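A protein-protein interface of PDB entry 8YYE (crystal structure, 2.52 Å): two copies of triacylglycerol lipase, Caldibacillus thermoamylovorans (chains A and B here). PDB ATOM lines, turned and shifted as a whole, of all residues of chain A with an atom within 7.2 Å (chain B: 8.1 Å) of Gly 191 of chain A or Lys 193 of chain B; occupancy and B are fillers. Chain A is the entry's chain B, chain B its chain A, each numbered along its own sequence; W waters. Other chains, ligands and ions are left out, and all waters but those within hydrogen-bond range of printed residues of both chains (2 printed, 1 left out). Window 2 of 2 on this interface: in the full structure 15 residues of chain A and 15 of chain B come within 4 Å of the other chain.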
ATOM      1  N   PHE A  23     -16.174 -33.083 -24.068  1.00  0.00           N
ATOM      2  CA  PHE A  23     -16.200 -31.620 -23.949  1.00  0.00           C
ATOM      3  C   PHE A  23     -16.937 -31.234 -22.680  1.00  0.00           C
ATOM      4  O   PHE A  23     -18.168 -31.295 -22.633  1.00  0.00           O
ATOM      5  CB  PHE A  23     -16.867 -30.961 -25.150  1.00  0.00           C
ATOM      6  CG  PHE A  23     -16.149 -31.192 -26.411  1.00  0.00           C
ATOM      7  CD1 PHE A  23     -15.011 -30.479 -26.705  1.00  0.00           C
ATOM      8  CD2 PHE A  23     -16.580 -32.159 -27.289  1.00  0.00           C
ATOM      9  CE1 PHE A  23     -14.326 -30.709 -27.874  1.00  0.00           C
ATOM     10  CE2 PHE A  23     -15.892 -32.409 -28.457  1.00  0.00           C
ATOM     11  CZ  PHE A  23     -14.766 -31.684 -28.753  1.00  0.00           C
ATOM     12  N   TYR A  26     -20.100 -28.598 -22.503  1.00  0.00           N
ATOM     13  CA  TYR A  26     -20.736 -28.462 -23.811  1.00  0.00           C
ATOM     14  C   TYR A  26     -21.197 -29.829 -24.297  1.00  0.00           C
ATOM     15  O   TYR A  26     -20.376 -30.684 -24.642  1.00  0.00           O
ATOM     16  CB  TYR A  26     -19.798 -27.809 -24.816  1.00  0.00           C
ATOM     17  CG  TYR A  26     -20.536 -27.306 -26.020  1.00  0.00           C
ATOM     18  CD1 TYR A  26     -21.298 -26.137 -25.972  1.00  0.00           C
ATOM     19  CD2 TYR A  26     -20.498 -28.009 -27.204  1.00  0.00           C
ATOM     20  CE1 TYR A  26     -21.982 -25.683 -27.088  1.00  0.00           C
ATOM     21  CE2 TYR A  26     -21.181 -27.560 -28.322  1.00  0.00           C
ATOM     22  CZ  TYR A  26     -21.918 -26.401 -28.259  1.00  0.00           C
ATOM     23  OH  TYR A  26     -22.596 -25.974 -29.383  1.00  0.00           O
ATOM     24  N   HIS A 185     -15.691 -25.446 -35.535  1.00  0.00           N
ATOM     25  CA  HIS A 185     -16.833 -24.817 -34.874  1.00  0.00           C
ATOM     26  C   HIS A 185     -17.105 -25.449 -33.514  1.00  0.00           C
ATOM     27  O   HIS A 185     -17.414 -24.748 -32.539  1.00  0.00           O
ATOM     28  CB  HIS A 185     -18.065 -24.914 -35.769  1.00  0.00           C
ATOM     29  CG  HIS A 185     -18.078 -23.903 -36.871  1.00  0.00           C
ATOM     30  ND1 HIS A 185     -17.211 -23.963 -37.942  1.00  0.00           N
ATOM     31  CD2 HIS A 185     -18.830 -22.791 -37.055  1.00  0.00           C
ATOM     32  CE1 HIS A 185     -17.440 -22.945 -38.749  1.00  0.00           C
ATOM     33  NE2 HIS A 185     -18.419 -22.220 -38.235  1.00  0.00           N
ATOM     34  N   LEU A 186     -16.957 -26.770 -33.420  1.00  0.00           N
ATOM     35  CA  LEU A 186     -17.250 -27.468 -32.176  1.00  0.00           C
ATOM     36  C   LEU A 186     -16.275 -27.066 -31.075  1.00  0.00           C
ATOM     37  O   LEU A 186     -16.689 -26.713 -29.963  1.00  0.00           O
ATOM     38  CB  LEU A 186     -17.220 -28.986 -32.408  1.00  0.00           C
ATOM     39  CG  LEU A 186     -17.106 -29.865 -31.160  1.00  0.00           C
ATOM     40  CD1 LEU A 186     -18.336 -29.656 -30.274  1.00  0.00           C
ATOM     41  CD2 LEU A 186     -16.985 -31.337 -31.575  1.00  0.00           C
ATOM     42  N   ALA A 187     -14.969 -27.136 -31.357  1.00  0.00           N
ATOM     43  CA  ALA A 187     -13.979 -26.659 -30.389  1.00  0.00           C
ATOM     44  C   ALA A 187     -14.284 -25.229 -29.951  1.00  0.00           C
ATOM     45  O   ALA A 187     -14.287 -24.924 -28.751  1.00  0.00           O
ATOM     46  CB  ALA A 187     -12.576 -26.755 -30.980  1.00  0.00           C
ATOM     47  N   SER A 188     -14.595 -24.354 -30.912  1.00  0.00           N
ATOM     48  CA  SER A 188     -14.897 -22.963 -30.600  1.00  0.00           C
ATOM     49  C   SER A 188     -16.107 -22.852 -29.683  1.00  0.00           C
ATOM     50  O   SER A 188     -16.053 -22.182 -28.643  1.00  0.00           O
ATOM     51  CB  SER A 188     -15.130 -22.187 -31.893  1.00  0.00           C
ATOM     52  OG  SER A 188     -15.539 -20.863 -31.609  1.00  0.00           O
ATOM     53  N   ALA A 189     -17.226 -23.471 -30.079  1.00  0.00           N
ATOM     54  CA  ALA A 189     -18.397 -23.523 -29.213  1.00  0.00           C
ATOM     55  C   ALA A 189     -18.032 -23.935 -27.798  1.00  0.00           C
ATOM     56  O   ALA A 189     -18.552 -23.360 -26.833  1.00  0.00           O
ATOM     57  CB  ALA A 189     -19.433 -24.492 -29.783  1.00  0.00           C
ATOM     58  N   ALA A 190     -17.132 -24.910 -27.663  1.00  0.00           N
ATOM     59  CA  ALA A 190     -16.746 -25.458 -26.375  1.00  0.00           C
ATOM     60  C   ALA A 190     -15.649 -24.655 -25.706  1.00  0.00           C
ATOM     61  O   ALA A 190     -15.190 -25.055 -24.636  1.00  0.00           O
ATOM     62  CB  ALA A 190     -16.286 -26.916 -26.525  1.00  0.00           C
ATOM     63  N   GLY A 191     -15.218 -23.547 -26.306  1.00  0.00           N
ATOM     64  CA  GLY A 191     -14.126 -22.756 -25.766  1.00  0.00           C
ATOM     65  C   GLY A 191     -12.836 -23.517 -25.529  1.00  0.00           C
ATOM     66  O   GLY A 191     -12.161 -23.267 -24.525  1.00  0.00           O
ATOM     67  N   GLN A 192     -12.465 -24.415 -26.446  1.00  0.00           N
ATOM     68  CA  GLN A 192     -11.305 -25.288 -26.292  1.00  0.00           C
ATOM     69  C   GLN A 192     -10.311 -25.070 -27.431  1.00  0.00           C
ATOM     70  O   GLN A 192     -10.703 -24.876 -28.586  1.00  0.00           O
ATOM     71  CB  GLN A 192     -11.765 -26.759 -26.234  1.00  0.00           C
ATOM     72  CG  GLN A 192     -10.726 -27.778 -25.773  1.00  0.00           C
ATOM     73  CD  GLN A 192     -11.367 -29.038 -25.175  1.00  0.00           C
ATOM     74  OE1 GLN A 192     -12.418 -28.968 -24.528  1.00  0.00           O
ATOM     75  NE2 GLN A 192     -10.724 -30.195 -25.384  1.00  0.00           N
ATOM     76  N   LYS A 193      -9.023 -25.090 -27.101  1.00  0.00           N
ATOM     77  CA  LYS A 193      -7.985 -24.937 -28.115  1.00  0.00           C
ATOM     78  C   LYS A 193      -7.897 -26.186 -28.983  1.00  0.00           C
ATOM     79  O   LYS A 193      -8.074 -27.307 -28.502  1.00  0.00           O
ATOM     80  CB  LYS A 193      -6.630 -24.666 -27.454  1.00  0.00           C
ATOM     81  CG  LYS A 193      -6.459 -23.238 -27.006  1.00  0.00           C
ATOM     82  CD  LYS A 193      -5.037 -22.891 -26.602  1.00  0.00           C
ATOM     83  CE  LYS A 193      -4.746 -23.364 -25.189  1.00  0.00           C
ATOM     84  NZ  LYS A 193      -3.508 -22.749 -24.625  1.00  0.00           N
ATOM     85  N   SER A 196      -5.528 -29.074 -27.769  1.00  0.00           N
ATOM     86  CA  SER A 196      -5.880 -29.814 -26.566  1.00  0.00           C
ATOM     87  C   SER A 196      -7.136 -30.669 -26.733  1.00  0.00           C
ATOM     88  O   SER A 196      -7.621 -31.242 -25.752  1.00  0.00           O
ATOM     89  CB  SER A 196      -6.033 -28.850 -25.394  1.00  0.00           C
ATOM     90  OG  SER A 196      -6.909 -27.801 -25.735  1.00  0.00           O
ATOM     91  N   LEU A 197      -7.649 -30.799 -27.951  1.00  0.00           N
ATOM     92  CA  LEU A 197      -8.845 -31.590 -28.183  1.00  0.00           C
ATOM     93  C   LEU A 197      -8.550 -33.062 -27.942  1.00  0.00           C
ATOM     94  O   LEU A 197      -7.481 -33.561 -28.310  1.00  0.00           O
ATOM     95  CB  LEU A 197      -9.342 -31.372 -29.606  1.00  0.00           C
ATOM     96  CG  LEU A 197     -10.648 -30.607 -29.791  1.00  0.00           C
ATOM     97  CD1 LEU A 197     -10.583 -29.283 -29.091  1.00  0.00           C
ATOM     98  CD2 LEU A 197     -10.828 -30.376 -31.280  1.00  0.00           C
ATOM     99  N   ILE A 359     -24.556 -23.745 -30.046  1.00  0.00           N
ATOM    100  CA  ILE A 359     -24.312 -22.339 -29.735  1.00  0.00           C
ATOM    101  C   ILE A 359     -24.789 -21.438 -30.871  1.00  0.00           C
ATOM    102  O   ILE A 359     -24.606 -21.738 -32.057  1.00  0.00           O
ATOM    103  CB  ILE A 359     -22.821 -22.126 -29.420  1.00  0.00           C
ATOM    104  CG1 ILE A 359     -22.573 -22.312 -27.929  1.00  0.00           C
ATOM    105  CG2 ILE A 359     -22.327 -20.763 -29.879  1.00  0.00           C
ATOM    106  CD1 ILE A 359     -21.110 -22.202 -27.579  1.00  0.00           C
ATOM    107  N   PHE B  23      -5.404  -9.777 -30.494  1.00  0.00           N
ATOM    108  CA  PHE B  23      -5.080 -11.175 -30.215  1.00  0.00           C
ATOM    109  C   PHE B  23      -3.638 -11.244 -29.751  1.00  0.00           C
ATOM    110  O   PHE B  23      -2.736 -10.849 -30.494  1.00  0.00           O
ATOM    111  CB  PHE B  23      -5.260 -12.042 -31.457  1.00  0.00           C
ATOM    112  CG  PHE B  23      -6.655 -12.088 -31.942  1.00  0.00           C
ATOM    113  CD1 PHE B  23      -7.591 -12.918 -31.320  1.00  0.00           C
ATOM    114  CD2 PHE B  23      -7.058 -11.263 -32.979  1.00  0.00           C
ATOM    115  CE1 PHE B  23      -8.900 -12.969 -31.749  1.00  0.00           C
ATOM    116  CE2 PHE B  23      -8.367 -11.297 -33.415  1.00  0.00           C
ATOM    117  CZ  PHE B  23      -9.292 -12.153 -32.797  1.00  0.00           C
ATOM    118  N   ALA B 187     -10.650 -16.683 -34.079  1.00  0.00           N
ATOM    119  CA  ALA B 187     -10.404 -16.990 -32.671  1.00  0.00           C
ATOM    120  C   ALA B 187      -9.802 -18.390 -32.498  1.00  0.00           C
ATOM    121  O   ALA B 187      -8.876 -18.589 -31.696  1.00  0.00           O
ATOM    122  CB  ALA B 187     -11.698 -16.844 -31.877  1.00  0.00           C
ATOM    123  N   SER B 188     -10.307 -19.368 -33.254  1.00  0.00           N
ATOM    124  CA  SER B 188      -9.739 -20.711 -33.218  1.00  0.00           C
ATOM    125  C   SER B 188      -8.257 -20.705 -33.566  1.00  0.00           C
ATOM    126  O   SER B 188      -7.450 -21.345 -32.886  1.00  0.00           O
ATOM    127  CB  SER B 188     -10.497 -21.625 -34.174  1.00  0.00           C
ATOM    128  OG  SER B 188      -9.827 -22.861 -34.289  1.00  0.00           O
ATOM    129  N   ALA B 190      -6.129 -18.325 -33.373  1.00  0.00           N
ATOM    130  CA  ALA B 190      -5.389 -17.617 -32.342  1.00  0.00           C
ATOM    131  C   ALA B 190      -5.355 -18.376 -31.024  1.00  0.00           C
ATOM    132  O   ALA B 190      -4.757 -17.894 -30.056  1.00  0.00           O
ATOM    133  CB  ALA B 190      -5.996 -16.230 -32.114  1.00  0.00           C
ATOM    134  N   GLY B 191      -5.990 -19.539 -30.957  1.00  0.00           N
ATOM    135  CA  GLY B 191      -6.039 -20.277 -29.711  1.00  0.00           C
ATOM    136  C   GLY B 191      -6.692 -19.518 -28.578  1.00  0.00           C
ATOM    137  O   GLY B 191      -6.258 -19.650 -27.429  1.00  0.00           O
ATOM    138  N   GLN B 192      -7.740 -18.739 -28.873  1.00  0.00           N
ATOM    139  CA  GLN B 192      -8.378 -17.862 -27.897  1.00  0.00           C
ATOM    140  C   GLN B 192      -9.860 -18.184 -27.745  1.00  0.00           C
ATOM    141  O   GLN B 192     -10.540 -18.504 -28.722  1.00  0.00           O
ATOM    142  CB  GLN B 192      -8.200 -16.393 -28.303  1.00  0.00           C
ATOM    143  CG  GLN B 192      -8.618 -15.377 -27.243  1.00  0.00           C
ATOM    144  CD  GLN B 192      -7.913 -14.056 -27.426  1.00  0.00           C
ATOM    145  OE1 GLN B 192      -6.746 -14.012 -27.835  1.00  0.00           O
ATOM    146  NE2 GLN B 192      -8.618 -12.965 -27.140  1.00  0.00           N
ATOM    147  N   LYS B 193     -10.359 -18.060 -26.518  1.00  0.00           N
ATOM    148  CA  LYS B 193     -11.750 -18.380 -26.215  1.00  0.00           C
ATOM    149  C   LYS B 193     -12.706 -17.283 -26.686  1.00  0.00           C
ATOM    150  O   LYS B 193     -12.491 -16.094 -26.431  1.00  0.00           O
ATOM    151  CB  LYS B 193     -11.932 -18.602 -24.706  1.00  0.00           C
ATOM    152  CG  LYS B 193     -11.457 -19.965 -24.189  1.00  0.00           C
ATOM    153  CD  LYS B 193     -11.944 -20.223 -22.754  1.00  0.00           C
ATOM    154  CE  LYS B 193     -11.182 -21.382 -22.093  1.00  0.00           C
ATOM    155  NZ  LYS B 193     -11.960 -22.058 -20.997  1.00  0.00           N
ATOM    156  N   GLN B 194     -13.795 -17.703 -27.347  1.00  0.00           N
ATOM    157  CA  GLN B 194     -14.813 -16.765 -27.826  1.00  0.00           C
ATOM    158  C   GLN B 194     -15.287 -15.839 -26.719  1.00  0.00           C
ATOM    159  O   GLN B 194     -15.604 -14.673 -26.974  1.00  0.00           O
ATOM    160  CB  GLN B 194     -16.014 -17.522 -28.402  1.00  0.00           C
ATOM    161  CG  GLN B 194     -15.799 -18.022 -29.819  1.00  0.00           C
ATOM    162  CD  GLN B 194     -15.881 -16.912 -30.854  1.00  0.00           C
ATOM    163  OE1 GLN B 194     -14.971 -16.745 -31.668  1.00  0.00           O
ATOM    164  NE2 GLN B 194     -16.976 -16.155 -30.837  1.00  0.00           N
ATOM    165  N   GLU B 195     -15.314 -16.330 -25.485  1.00  0.00           N
ATOM    166  CA  GLU B 195     -15.892 -15.565 -24.392  1.00  0.00           C
ATOM    167  C   GLU B 195     -14.976 -14.436 -23.961  1.00  0.00           C
ATOM    168  O   GLU B 195     -15.442 -13.468 -23.356  1.00  0.00           O
ATOM    169  CB  GLU B 195     -16.177 -16.497 -23.216  1.00  0.00           C
ATOM    170  CG  GLU B 195     -17.226 -17.561 -23.527  1.00  0.00           C
ATOM    171  CD  GLU B 195     -16.632 -18.759 -24.294  1.00  0.00           C
ATOM    172  OE1 GLU B 195     -15.500 -19.185 -23.962  1.00  0.00           O
ATOM    173  OE2 GLU B 195     -17.296 -19.276 -25.227  1.00  0.00           O
ATOM    174  N   SER B 196     -13.681 -14.538 -24.255  1.00  0.00           N
ATOM    175  CA  SER B 196     -12.707 -13.545 -23.824  1.00  0.00           C
ATOM    176  C   SER B 196     -12.230 -12.653 -24.966  1.00  0.00           C
ATOM    177  O   SER B 196     -11.278 -11.894 -24.781  1.00  0.00           O
ATOM    178  CB  SER B 196     -11.510 -14.236 -23.173  1.00  0.00           C
ATOM    179  OG  SER B 196     -10.958 -15.205 -24.053  1.00  0.00           O
ATOM    180  N   LEU B 197     -12.861 -12.744 -26.138  1.00  0.00           N
ATOM    181  CA  LEU B 197     -12.493 -11.930 -27.290  1.00  0.00           C
ATOM    182  C   LEU B 197     -12.745 -10.451 -27.034  1.00  0.00           C
ATOM    183  O   LEU B 197     -13.822 -10.058 -26.574  1.00  0.00           O
ATOM    184  CB  LEU B 197     -13.286 -12.384 -28.516  1.00  0.00           C
ATOM    185  CG  LEU B 197     -12.624 -13.225 -29.618  1.00  0.00           C
ATOM    186  CD1 LEU B 197     -11.610 -14.253 -29.113  1.00  0.00           C
ATOM    187  CD2 LEU B 197     -13.700 -13.915 -30.463  1.00  0.00           C
ATOM    188  N   ILE B 198     -11.741  -9.630 -27.351  1.00  0.00           N
ATOM    189  CA  ILE B 198     -11.890  -8.179 -27.351  1.00  0.00           C
ATOM    190  C   ILE B 198     -11.769  -7.663 -28.781  1.00  0.00           C
ATOM    191  O   ILE B 198     -11.363  -6.516 -29.008  1.00  0.00           O
ATOM    192  CB  ILE B 198     -10.853  -7.517 -26.431  1.00  0.00           C
ATOM    193  CG1 ILE B 198      -9.439  -7.865 -26.892  1.00  0.00           C
ATOM    194  CG2 ILE B 198     -11.078  -7.972 -24.997  1.00  0.00           C
ATOM    195  CD1 ILE B 198      -8.378  -6.843 -26.520  1.00  0.00           C
ATOM    196  N   PHE B 216     -18.979 -10.443 -25.219  1.00  0.00           N
ATOM    197  CA  PHE B 216     -18.591 -10.350 -26.620  1.00  0.00           C
ATOM    198  C   PHE B 216     -19.701 -10.832 -27.541  1.00  0.00           C
ATOM    199  O   PHE B 216     -19.971 -10.201 -28.566  1.00  0.00           O
ATOM    200  CB  PHE B 216     -17.326 -11.144 -26.905  1.00  0.00           C
ATOM    201  CG  PHE B 216     -16.933 -11.091 -28.332  1.00  0.00           C
ATOM    202  CD1 PHE B 216     -16.361  -9.937 -28.850  1.00  0.00           C
ATOM    203  CD2 PHE B 216     -17.183 -12.154 -29.180  1.00  0.00           C
ATOM    204  CE1 PHE B 216     -15.996  -9.850 -30.204  1.00  0.00           C
ATOM    205  CE2 PHE B 216     -16.830 -12.079 -30.529  1.00  0.00           C
ATOM    206  CZ  PHE B 216     -16.234 -10.925 -31.041  1.00  0.00           C
HETATM  207  O   HOH W   1     -13.410 -19.649 -32.162  1.00  0.00           O
HETATM  208  O   HOH W   2     -13.866 -20.422 -27.993  1.00  0.00           O
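The backbone carbonyl oxygen of Lys 193 of chain B sits at hydrogen-bond distance from the side-chain hydroxyl of Ser 196 of chain B (3.0 Å). OG of Ser 196 of chain A lies within hydrogen-bond range of O of Lys 193 of chain A.
OG of Ser 188 of chain A touches CG of Gln 194 of chain B, at 3.4 Å. O of Gly 191 of chain A touches CE of Lys 193 of chain B, at 3.2 Å. CD of Lys 193 of chain A touches O of Gly 191 of chain B (3.6 Å).
Leu 186 of chain A touches none of the printed residues of chain B. Of the printed residues of chain B, Ser 188 of chain A touches Gln 194 (3.4 Å). No residue of chain B comes within 4 Å of Ala 190 of chain A. Gly 191 of chain A touches just one residue of chain B: Lys 193 (3.2 Å). Of the printed residues of chain A, Gly 191 of chain B touches Lys 193 (3.6 Å). Of the printed residues of chain A, Lys 193 of chain B touches Gly 191. Phe 216 of chain B touches none of the printed residues of chain A. The nearest residue of chain A that does not touch Lys 193 of chain B is Gln 192 of chain A (5.1 Å). The nearest printed residue of chain B that does not touch Ser 188 of chain A is Glu 195 of chain B (4.7 Å).
Printed residues of chain B that touch a printed residue of chain A: Gly 191, Lys 193 and Gln 194. Along chain B the printed residues that touch a printed residue of chain A span positions 191 to 194. Among the printed residues, no Asp or Glu carboxylate lies within 4 Å of a Lys or Arg side-chain nitrogen of the other chain.
Gly 191 of chain A touches Lys 193 of chain B, and with the chains exchanged Lys 193 of chain A touches Gly 191 of chain B. Of the 3 pairs that touch across the chains among the printed residues, 2 have their exchanged pair printed and touching as well.
Water W1 lies within hydrogen-bond range of the side-chain hydroxyl (OG) of Ser 188 of chain A (2.5 Å), the backbone NH (N) of Ser 188 of chain B (3.3 Å) and the side-chain amide oxygen (OE1) of Gln 194 of chain B (3.3 Å). Water W2 lies within hydrogen-bond range of the backbone NH (N) of Gln 194 of chain B and the backbone carbonyl oxygen (O) of Ser 188 of chain A.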
